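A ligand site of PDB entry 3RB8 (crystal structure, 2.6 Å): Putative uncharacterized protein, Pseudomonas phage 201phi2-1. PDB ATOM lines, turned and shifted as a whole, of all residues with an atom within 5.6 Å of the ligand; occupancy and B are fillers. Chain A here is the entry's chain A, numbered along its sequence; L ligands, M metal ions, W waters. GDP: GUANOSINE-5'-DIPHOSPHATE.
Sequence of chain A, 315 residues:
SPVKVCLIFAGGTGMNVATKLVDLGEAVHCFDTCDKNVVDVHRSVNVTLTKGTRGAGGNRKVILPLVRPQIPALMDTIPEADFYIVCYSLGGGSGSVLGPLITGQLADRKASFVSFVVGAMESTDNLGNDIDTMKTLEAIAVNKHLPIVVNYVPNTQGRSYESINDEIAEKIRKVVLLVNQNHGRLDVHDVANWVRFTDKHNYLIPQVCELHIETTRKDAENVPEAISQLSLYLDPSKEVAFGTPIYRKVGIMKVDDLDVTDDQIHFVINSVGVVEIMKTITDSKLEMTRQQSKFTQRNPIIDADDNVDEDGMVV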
ATOM      1  N   ALA A  10       9.270  -1.306  -4.281  1.00  0.00           N
ATOM      2  CA  ALA A  10       7.857  -1.624  -4.488  1.00  0.00           C
ATOM      3  C   ALA A  10       7.014  -0.440  -4.979  1.00  0.00           C
ATOM      4  O   ALA A  10       7.153   0.687  -4.497  1.00  0.00           O
ATOM      5  CB  ALA A  10       7.280  -2.207  -3.233  1.00  0.00           C
ATOM      6  N   GLY A  11       6.121  -0.720  -5.926  1.00  0.00           N
ATOM      7  CA  GLY A  11       5.214   0.270  -6.482  1.00  0.00           C
ATOM      8  C   GLY A  11       5.857   1.119  -7.572  1.00  0.00           C
ATOM      9  O   GLY A  11       7.004   0.881  -7.974  1.00  0.00           O
ATOM     10  N   GLY A  12       5.117   2.129  -8.026  1.00  0.00           N
ATOM     11  CA  GLY A  12       5.571   3.001  -9.089  1.00  0.00           C
ATOM     12  C   GLY A  12       6.858   3.718  -8.762  1.00  0.00           C
ATOM     13  O   GLY A  12       7.887   3.517  -9.414  1.00  0.00           O
ATOM     14  N   THR A  13       6.801   4.558  -7.731  1.00  0.00           N
ATOM     15  CA  THR A  13       7.980   5.283  -7.267  1.00  0.00           C
ATOM     16  C   THR A  13       9.147   4.323  -7.100  1.00  0.00           C
ATOM     17  O   THR A  13      10.256   4.606  -7.547  1.00  0.00           O
ATOM     18  CB  THR A  13       7.703   5.967  -5.925  1.00  0.00           C
ATOM     19  OG1 THR A  13       6.626   6.893  -6.087  1.00  0.00           O
ATOM     20  CG2 THR A  13       8.912   6.708  -5.457  1.00  0.00           C
ATOM     21  N   GLY A  14       8.867   3.186  -6.464  1.00  0.00           N
ATOM     22  CA  GLY A  14       9.881   2.183  -6.213  1.00  0.00           C
ATOM     23  C   GLY A  14      10.621   1.747  -7.472  1.00  0.00           C
ATOM     24  O   GLY A  14      11.844   1.638  -7.472  1.00  0.00           O
ATOM     25  N   ASN A  16      10.520   3.269 -10.556  1.00  0.00           N
ATOM     26  CA  ASN A  16      11.153   4.457 -11.119  1.00  0.00           C
ATOM     27  C   ASN A  16      12.552   4.753 -10.505  1.00  0.00           C
ATOM     28  O   ASN A  16      13.486   5.106 -11.218  1.00  0.00           O
ATOM     29  CB  ASN A  16      10.211   5.648 -10.985  1.00  0.00           C
ATOM     30  CG  ASN A  16       8.895   5.421 -11.700  1.00  0.00           C
ATOM     31  OD1 ASN A  16       8.750   4.466 -12.489  1.00  0.00           O
ATOM     32  ND2 ASN A  16       7.922   6.289 -11.453  1.00  0.00           N
ATOM     33  N   VAL A  17      12.664   4.592  -9.193  1.00  0.00           N
ATOM     34  CA  VAL A  17      13.941   4.728  -8.509  1.00  0.00           C
ATOM     35  C   VAL A  17      14.842   3.551  -8.883  1.00  0.00           C
ATOM     36  O   VAL A  17      16.078   3.655  -8.861  1.00  0.00           O
ATOM     37  CB  VAL A  17      13.756   4.766  -6.966  1.00  0.00           C
ATOM     38  CG1 VAL A  17      15.074   4.929  -6.251  1.00  0.00           C
ATOM     39  CG2 VAL A  17      12.803   5.875  -6.559  1.00  0.00           C
ATOM     40  N   ASP A  32       5.384  -5.038  -7.934  1.00  0.00           N
ATOM     41  CA  ASP A  32       4.246  -4.132  -8.047  1.00  0.00           C
ATOM     42  C   ASP A  32       2.956  -4.962  -8.143  1.00  0.00           C
ATOM     43  O   ASP A  32       2.995  -6.183  -8.075  1.00  0.00           O
ATOM     44  CB  ASP A  32       4.411  -3.171  -9.241  1.00  0.00           C
ATOM     45  CG  ASP A  32       3.548  -1.897  -9.097  1.00  0.00           C
ATOM     46  OD1 ASP A  32       3.741  -0.947  -9.899  1.00  0.00           O
ATOM     47  OD2 ASP A  32       2.689  -1.827  -8.186  1.00  0.00           O
ATOM     48  N   ASN A  37       4.661   0.554 -14.517  1.00  0.00           N
ATOM     49  CA  ASN A  37       5.979   1.189 -14.484  1.00  0.00           C
ATOM     50  C   ASN A  37       7.131   0.295 -14.932  1.00  0.00           C
ATOM     51  O   ASN A  37       8.308   0.624 -14.676  1.00  0.00           O
ATOM     52  CB  ASN A  37       6.272   1.718 -13.074  1.00  0.00           C
ATOM     53  CG  ASN A  37       5.274   2.765 -12.627  1.00  0.00           C
ATOM     54  OD1 ASN A  37       4.132   2.448 -12.287  1.00  0.00           O
ATOM     55  ND2 ASN A  37       5.708   4.025 -12.627  1.00  0.00           N
ATOM     56  N   GLY A  57      -5.834   0.850  -7.231  1.00  0.00           N
ATOM     57  CA  GLY A  57      -5.543   1.853  -6.201  1.00  0.00           C
ATOM     58  C   GLY A  57      -4.070   2.214  -6.012  1.00  0.00           C
ATOM     59  O   GLY A  57      -3.148   1.470  -6.384  1.00  0.00           O
ATOM     60  N   GLY A  58      -3.839   3.350  -5.374  1.00  0.00           N
ATOM     61  CA  GLY A  58      -4.897   4.153  -4.822  1.00  0.00           C
ATOM     62  C   GLY A  58      -5.196   3.725  -3.400  1.00  0.00           C
ATOM     63  O   GLY A  58      -4.702   4.318  -2.423  1.00  0.00           O
ATOM     64  N   SER A  89       7.029   4.504  -2.172  1.00  0.00           N
ATOM     65  CA  SER A  89       6.326   5.710  -1.762  1.00  0.00           C
ATOM     66  C   SER A  89       5.317   5.398  -0.654  1.00  0.00           C
ATOM     67  O   SER A  89       4.693   4.346  -0.667  1.00  0.00           O
ATOM     68  CB  SER A  89       5.584   6.309  -2.962  1.00  0.00           C
ATOM     69  OG  SER A  89       4.830   7.453  -2.600  1.00  0.00           O
ATOM     70  N   GLY A  91       2.756   7.269  -0.466  1.00  0.00           N
ATOM     71  CA  GLY A  91       1.563   7.905  -1.009  1.00  0.00           C
ATOM     72  C   GLY A  91       0.586   7.048  -1.803  1.00  0.00           C
ATOM     73  O   GLY A  91      -0.626   7.273  -1.710  1.00  0.00           O
ATOM     74  N   GLY A  92       1.098   6.100  -2.584  1.00  0.00           N
ATOM     75  CA  GLY A  92       0.254   5.248  -3.407  1.00  0.00           C
ATOM     76  C   GLY A  92      -0.459   4.115  -2.669  1.00  0.00           C
ATOM     77  O   GLY A  92      -0.590   4.119  -1.442  1.00  0.00           O
ATOM     78  N   GLY A  93      -0.938   3.139  -3.438  1.00  0.00           N
ATOM     79  CA  GLY A  93      -1.646   2.002  -2.874  1.00  0.00           C
ATOM     80  C   GLY A  93      -0.838   0.709  -2.826  1.00  0.00           C
ATOM     81  O   GLY A  93      -1.019  -0.115  -1.927  1.00  0.00           O
ATOM     82  N   SER A  94       0.072   0.533  -3.785  1.00  0.00           N
ATOM     83  CA  SER A  94       0.824  -0.722  -3.916  1.00  0.00           C
ATOM     84  C   SER A  94       2.154  -0.742  -3.139  1.00  0.00           C
ATOM     85  O   SER A  94       2.391  -1.651  -2.349  1.00  0.00           O
ATOM     86  CB  SER A  94       1.038  -1.087  -5.388  1.00  0.00           C
ATOM     87  OG  SER A  94      -0.208  -1.298  -6.049  1.00  0.00           O
ATOM     88  N   GLY A  95       3.001   0.265  -3.374  1.00  0.00           N
ATOM     89  CA  GLY A  95       4.233   0.397  -2.635  1.00  0.00           C
ATOM     90  C   GLY A  95       4.019   0.476  -1.136  1.00  0.00           C
ATOM     91  O   GLY A  95       4.701  -0.202  -0.365  1.00  0.00           O
ATOM     92  N   SER A  96       3.064   1.307  -0.730  1.00  0.00           N
ATOM     93  CA  SER A  96       2.755   1.530   0.691  1.00  0.00           C
ATOM     94  C   SER A  96       2.079   0.325   1.348  1.00  0.00           C
ATOM     95  O   SER A  96       1.717   0.352   2.522  1.00  0.00           O
ATOM     96  CB  SER A  96       1.877   2.764   0.866  1.00  0.00           C
ATOM     97  OG  SER A  96       0.659   2.602   0.146  1.00  0.00           O
ATOM     98  N   VAL A 118       9.251   8.077   0.165  1.00  0.00           N
ATOM     99  CA  VAL A 118       8.830   9.392  -0.350  1.00  0.00           C
ATOM    100  C   VAL A 118       7.506   9.840   0.272  1.00  0.00           C
ATOM    101  O   VAL A 118       6.517   9.090   0.276  1.00  0.00           O
ATOM    102  CB  VAL A 118       8.584   9.305  -1.884  1.00  0.00           C
ATOM    103  CG1 VAL A 118       7.880  10.560  -2.411  1.00  0.00           C
ATOM    104  CG2 VAL A 118       9.866   9.002  -2.633  1.00  0.00           C
ATOM    105  N   ALA A 120       4.530  11.581  -0.620  1.00  0.00           N
ATOM    106  CA  ALA A 120       3.708  12.062  -1.730  1.00  0.00           C
ATOM    107  C   ALA A 120       2.796  13.212  -1.304  1.00  0.00           C
ATOM    108  O   ALA A 120       2.165  13.131  -0.250  1.00  0.00           O
ATOM    109  CB  ALA A 120       2.856  10.917  -2.288  1.00  0.00           C
ATOM    110  N   MET A 121       2.690  14.265  -2.119  1.00  0.00           N
ATOM    111  CA  MET A 121       1.978  15.462  -1.651  1.00  0.00           C
ATOM    112  C   MET A 121       0.908  16.041  -2.590  1.00  0.00           C
ATOM    113  O   MET A 121       0.474  17.183  -2.392  1.00  0.00           O
ATOM    114  CB  MET A 121       2.988  16.539  -1.254  1.00  0.00           C
ATOM    115  CG  MET A 121       4.135  15.991  -0.428  1.00  0.00           C
ATOM    116  SD  MET A 121       4.443  16.927   1.246  1.00  0.00           S
ATOM    117  CE  MET A 121       5.562  18.401   0.589  1.00  0.00           C
ATOM    118  N   GLU A 122       0.489  15.264  -3.585  1.00  0.00           N
ATOM    119  CA  GLU A 122      -0.523  15.710  -4.561  1.00  0.00           C
ATOM    120  C   GLU A 122      -1.916  15.948  -3.956  1.00  0.00           C
ATOM    121  O   GLU A 122      -2.499  17.008  -4.145  1.00  0.00           O
ATOM    122  CB  GLU A 122      -0.641  14.724  -5.730  1.00  0.00           C
ATOM    123  CG  GLU A 122       0.586  14.596  -6.624  1.00  0.00           C
ATOM    124  CD  GLU A 122       0.364  13.617  -7.777  1.00  0.00           C
ATOM    125  OE1 GLU A 122      -0.712  12.957  -7.789  1.00  0.00           O
ATOM    126  OE2 GLU A 122       1.241  13.482  -8.660  1.00  0.00           O
ATOM    127  N   ASN A 126      -2.906  11.095  -1.162  1.00  0.00           N
ATOM    128  CA  ASN A 126      -1.489  10.985  -0.919  1.00  0.00           C
ATOM    129  C   ASN A 126      -1.142  11.255   0.547  1.00  0.00           C
ATOM    130  O   ASN A 126      -0.488  10.440   1.202  1.00  0.00           O
ATOM    131  CB  ASN A 126      -0.734  11.958  -1.821  1.00  0.00           C
ATOM    132  CG  ASN A 126      -0.548  11.433  -3.222  1.00  0.00           C
ATOM    133  OD1 ASN A 126      -0.021  12.125  -4.098  1.00  0.00           O
ATOM    134  ND2 ASN A 126      -0.986  10.201  -3.452  1.00  0.00           N
ATOM    135  N   ASN A 155       8.078  14.984  -1.265  1.00  0.00           N
ATOM    136  CA  ASN A 155       7.991  15.557  -2.605  1.00  0.00           C
ATOM    137  C   ASN A 155       7.750  17.056  -2.486  1.00  0.00           C
ATOM    138  O   ASN A 155       6.612  17.527  -2.513  1.00  0.00           O
ATOM    139  CB  ASN A 155       6.878  14.893  -3.419  1.00  0.00           C
ATOM    140  CG  ASN A 155       7.291  13.552  -3.988  1.00  0.00           C
ATOM    141  OD1 ASN A 155       8.482  13.249  -4.093  1.00  0.00           O
ATOM    142  ND2 ASN A 155       6.313  12.740  -4.360  1.00  0.00           N
ATOM    143  N   TYR A 161       9.778  14.968  -9.799  1.00  0.00           N
ATOM    144  CA  TYR A 161      10.035  13.610  -9.319  1.00  0.00           C
ATOM    145  C   TYR A 161      11.352  13.100  -9.881  1.00  0.00           C
ATOM    146  O   TYR A 161      12.053  12.302  -9.260  1.00  0.00           O
ATOM    147  CB  TYR A 161       8.922  12.628  -9.676  1.00  0.00           C
ATOM    148  CG  TYR A 161       7.561  12.986  -9.151  1.00  0.00           C
ATOM    149  CD1 TYR A 161       7.411  13.896  -8.105  1.00  0.00           C
ATOM    150  CD2 TYR A 161       6.410  12.440  -9.711  1.00  0.00           C
ATOM    151  CE1 TYR A 161       6.157  14.240  -7.636  1.00  0.00           C
ATOM    152  CE2 TYR A 161       5.147  12.764  -9.242  1.00  0.00           C
ATOM    153  CZ  TYR A 161       5.024  13.662  -8.201  1.00  0.00           C
ATOM    154  OH  TYR A 161       3.770  13.992  -7.723  1.00  0.00           O
ATOM    155  N   ILE A 164      13.855  14.443  -7.474  1.00  0.00           N
ATOM    156  CA  ILE A 164      13.698  13.754  -6.206  1.00  0.00           C
ATOM    157  C   ILE A 164      14.197  12.316  -6.280  1.00  0.00           C
ATOM    158  O   ILE A 164      15.032  11.901  -5.486  1.00  0.00           O
ATOM    159  CB  ILE A 164      12.255  13.804  -5.747  1.00  0.00           C
ATOM    160  CG1 ILE A 164      11.934  15.210  -5.244  1.00  0.00           C
ATOM    161  CG2 ILE A 164      12.026  12.802  -4.661  1.00  0.00           C
ATOM    162  CD1 ILE A 164      10.440  15.485  -5.078  1.00  0.00           C
ATOM    163  N   ASN A 165      13.710  11.564  -7.262  1.00  0.00           N
ATOM    164  CA  ASN A 165      14.208  10.208  -7.511  1.00  0.00           C
ATOM    165  C   ASN A 165      15.732  10.174  -7.645  1.00  0.00           C
ATOM    166  O   ASN A 165      16.374   9.215  -7.213  1.00  0.00           O
ATOM    167  CB  ASN A 165      13.615   9.626  -8.794  1.00  0.00           C
ATOM    168  CG  ASN A 165      12.164   9.230  -8.644  1.00  0.00           C
ATOM    169  OD1 ASN A 165      11.521   9.470  -7.618  1.00  0.00           O
ATOM    170  ND2 ASN A 165      11.632   8.612  -9.688  1.00  0.00           N
ATOM    171  N   ILE A 168      17.617  10.205  -4.321  1.00  0.00           N
ATOM    172  CA  ILE A 168      17.355   8.956  -3.614  1.00  0.00           C
ATOM    173  C   ILE A 168      18.314   7.894  -4.154  1.00  0.00           C
ATOM    174  O   ILE A 168      18.927   7.163  -3.391  1.00  0.00           O
ATOM    175  CB  ILE A 168      15.881   8.471  -3.779  1.00  0.00           C
ATOM    176  CG1 ILE A 168      14.902   9.448  -3.140  1.00  0.00           C
ATOM    177  CG2 ILE A 168      15.688   7.076  -3.196  1.00  0.00           C
ATOM    178  CD1 ILE A 168      13.455   9.043  -3.332  1.00  0.00           C
HETATM  179  PB  GDP L   1       1.969   2.825  -5.980  1.00  0.00           P
HETATM  180  O1B GDP L   1       2.648   2.133  -7.123  1.00  0.00           O
HETATM  181  O2B GDP L   1       2.606   2.286  -4.736  1.00  0.00           O
HETATM  182  O3B GDP L   1       0.508   2.503  -5.915  1.00  0.00           O
HETATM  183  O3A GDP L   1       2.087   4.433  -6.017  1.00  0.00           O
HETATM  184  PA  GDP L   1       3.074   5.301  -6.941  1.00  0.00           P
HETATM  185  O1A GDP L   1       2.854   5.025  -8.401  1.00  0.00           O
HETATM  186  O2A GDP L   1       4.507   5.022  -6.586  1.00  0.00           O
HETATM  187  O5' GDP L   1       2.652   6.821  -6.639  1.00  0.00           O
HETATM  188  C5' GDP L   1       2.281   7.284  -5.339  1.00  0.00           C
HETATM  189  C4' GDP L   1       2.524   8.786  -5.234  1.00  0.00           C
HETATM  190  O4' GDP L   1       3.910   9.109  -5.339  1.00  0.00           O
HETATM  191  C3' GDP L   1       1.852   9.579  -6.310  1.00  0.00           C
HETATM  192  O3' GDP L   1       0.617   9.995  -5.779  1.00  0.00           O
HETATM  193  C2' GDP L   1       2.749  10.770  -6.482  1.00  0.00           C
HETATM  194  O2' GDP L   1       2.451  11.653  -5.399  1.00  0.00           O
HETATM  195  C1' GDP L   1       4.142  10.280  -6.147  1.00  0.00           C
HETATM  196  N9  GDP L   1       5.001   9.712  -7.220  1.00  0.00           N
HETATM  197  C8  GDP L   1       4.628   8.905  -8.235  1.00  0.00           C
HETATM  198  N7  GDP L   1       5.713   8.517  -8.950  1.00  0.00           N
HETATM  199  C5  GDP L   1       6.815   9.050  -8.369  1.00  0.00           C
HETATM  200  C6  GDP L   1       8.283   9.033  -8.592  1.00  0.00           C
HETATM  201  O6  GDP L   1       8.793   8.396  -9.533  1.00  0.00           O
HETATM  202  N1  GDP L   1       9.052   9.723  -7.739  1.00  0.00           N
HETATM  203  C2  GDP L   1       8.555  10.411  -6.706  1.00  0.00           C
HETATM  204  N2  GDP L   1       9.420  11.079  -5.882  1.00  0.00           N
HETATM  205  N3  GDP L   1       7.231  10.471  -6.439  1.00  0.00           N
HETATM  206  C4  GDP L   1       6.322   9.824  -7.215  1.00  0.00           C
HETATM  207 MG    MG M   1       1.342   2.148  -9.609  1.00  0.00          MG
HETATM  208  O   HOH W   1       2.584   3.653  -2.626  1.00  0.00           O
HETATM  209  O   HOH W   2       0.860   0.004  -8.523  1.00  0.00           O
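The side-chain amide oxygen (OD1) of Asn 165 sits close to the backbone carbonyl oxygen (O) of Tyr 161. OD1 of Asn 16 lies close to O of Gly 12, 3.3 Å away. The side-chain amide oxygen (OD1) of Asn 126 lies close to the backbone NH (N) of Glu 122 (3.2 Å). ND2 of Asn 126 lies within hydrogen-bond range of O of Gly 91 (3.4 Å). ND2 of Asn 37 is in hydrogen-bond range of OD1 of Asn 16 (3.1 Å). OG of Ser 96 is in hydrogen-bond range of O of Gly 92 (2.5 Å). N of Ser 96 is in hydrogen-bond range of O of Ser 89 (3.4 Å). OE2 of Glu 122 is in hydrogen-bond range of OH of Tyr 161, at 2.7 Å.
The backbone NH of Gly 95 lies within hydrogen-bond range of an oxygen (O2B) of the ligand, at 2.5 Å. The side-chain amide oxygen (OD1) of Asn 165 lies within hydrogen-bond range of a nitrogen (N1) of the ligand. N of Thr 13 is in hydrogen-bond range of O2A of the ligand, 2.6 Å away. The side-chain hydroxyl of Thr 13 lies within hydrogen-bond range of an oxygen (O2A) of the ligand (2.9 Å). N of Gly 12 is in hydrogen-bond range of O1B of the ligand (2.6 Å). The side-chain amide oxygen of Asn 126 is in hydrogen-bond range of an oxygen (O3') of the ligand (2.8 Å). The backbone NH of Ser 94 lies within hydrogen-bond range of an oxygen (O3B) of the ligand (2.9 Å). N of Gly 93 is in hydrogen-bond range of O3B of the ligand (2.9 Å). The side-chain amide oxygen (OD1) of Asn 155 is in hydrogen-bond range of a nitrogen (N2) of the ligand, at 3.0 Å. The side-chain amide nitrogen of Asn 16 lies within hydrogen-bond range of an oxygen (O6) of the ligand (3.0 Å). The side-chain hydroxyl (OG) of Ser 89 lies within hydrogen-bond range of an oxygen (O4') of the ligand (3.3 Å).
Water W2 lies within hydrogen-bond range of the side-chain carboxylate (OD2) of Asp 32, the side-chain hydroxyl (OG) of Ser 94 and an oxygen (O1B) of the ligand.
CA of Gly 11 touches O1B of the ligand, at 3.2 Å. O of Gly 57 touches O3B of the ligand (3.8 Å). Gly 91 touches the ligand. Gly 92 touches the ligand (N to C5', 3.2 Å). CG1 of Val 118 touches N2 of the ligand (3.8 Å). Ala 120 touches the ligand. CG of Glu 122 touches O2' of the ligand, at 3.7 Å. CB of Tyr 161 touches N1 of the ligand, at 3.5 Å. Ile 164 touches the ligand (CG2 to N2, 3.4 Å). Hydrophobic or aromatic side chains that line the ligand: Val 118, Ala 120, Tyr 161 and Ile 164. Of the 28 residues printed, 19 come within 4 Å of the ligand. The nearest printed residue that does not touch the ligand is Asp 32 (4.1 Å).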
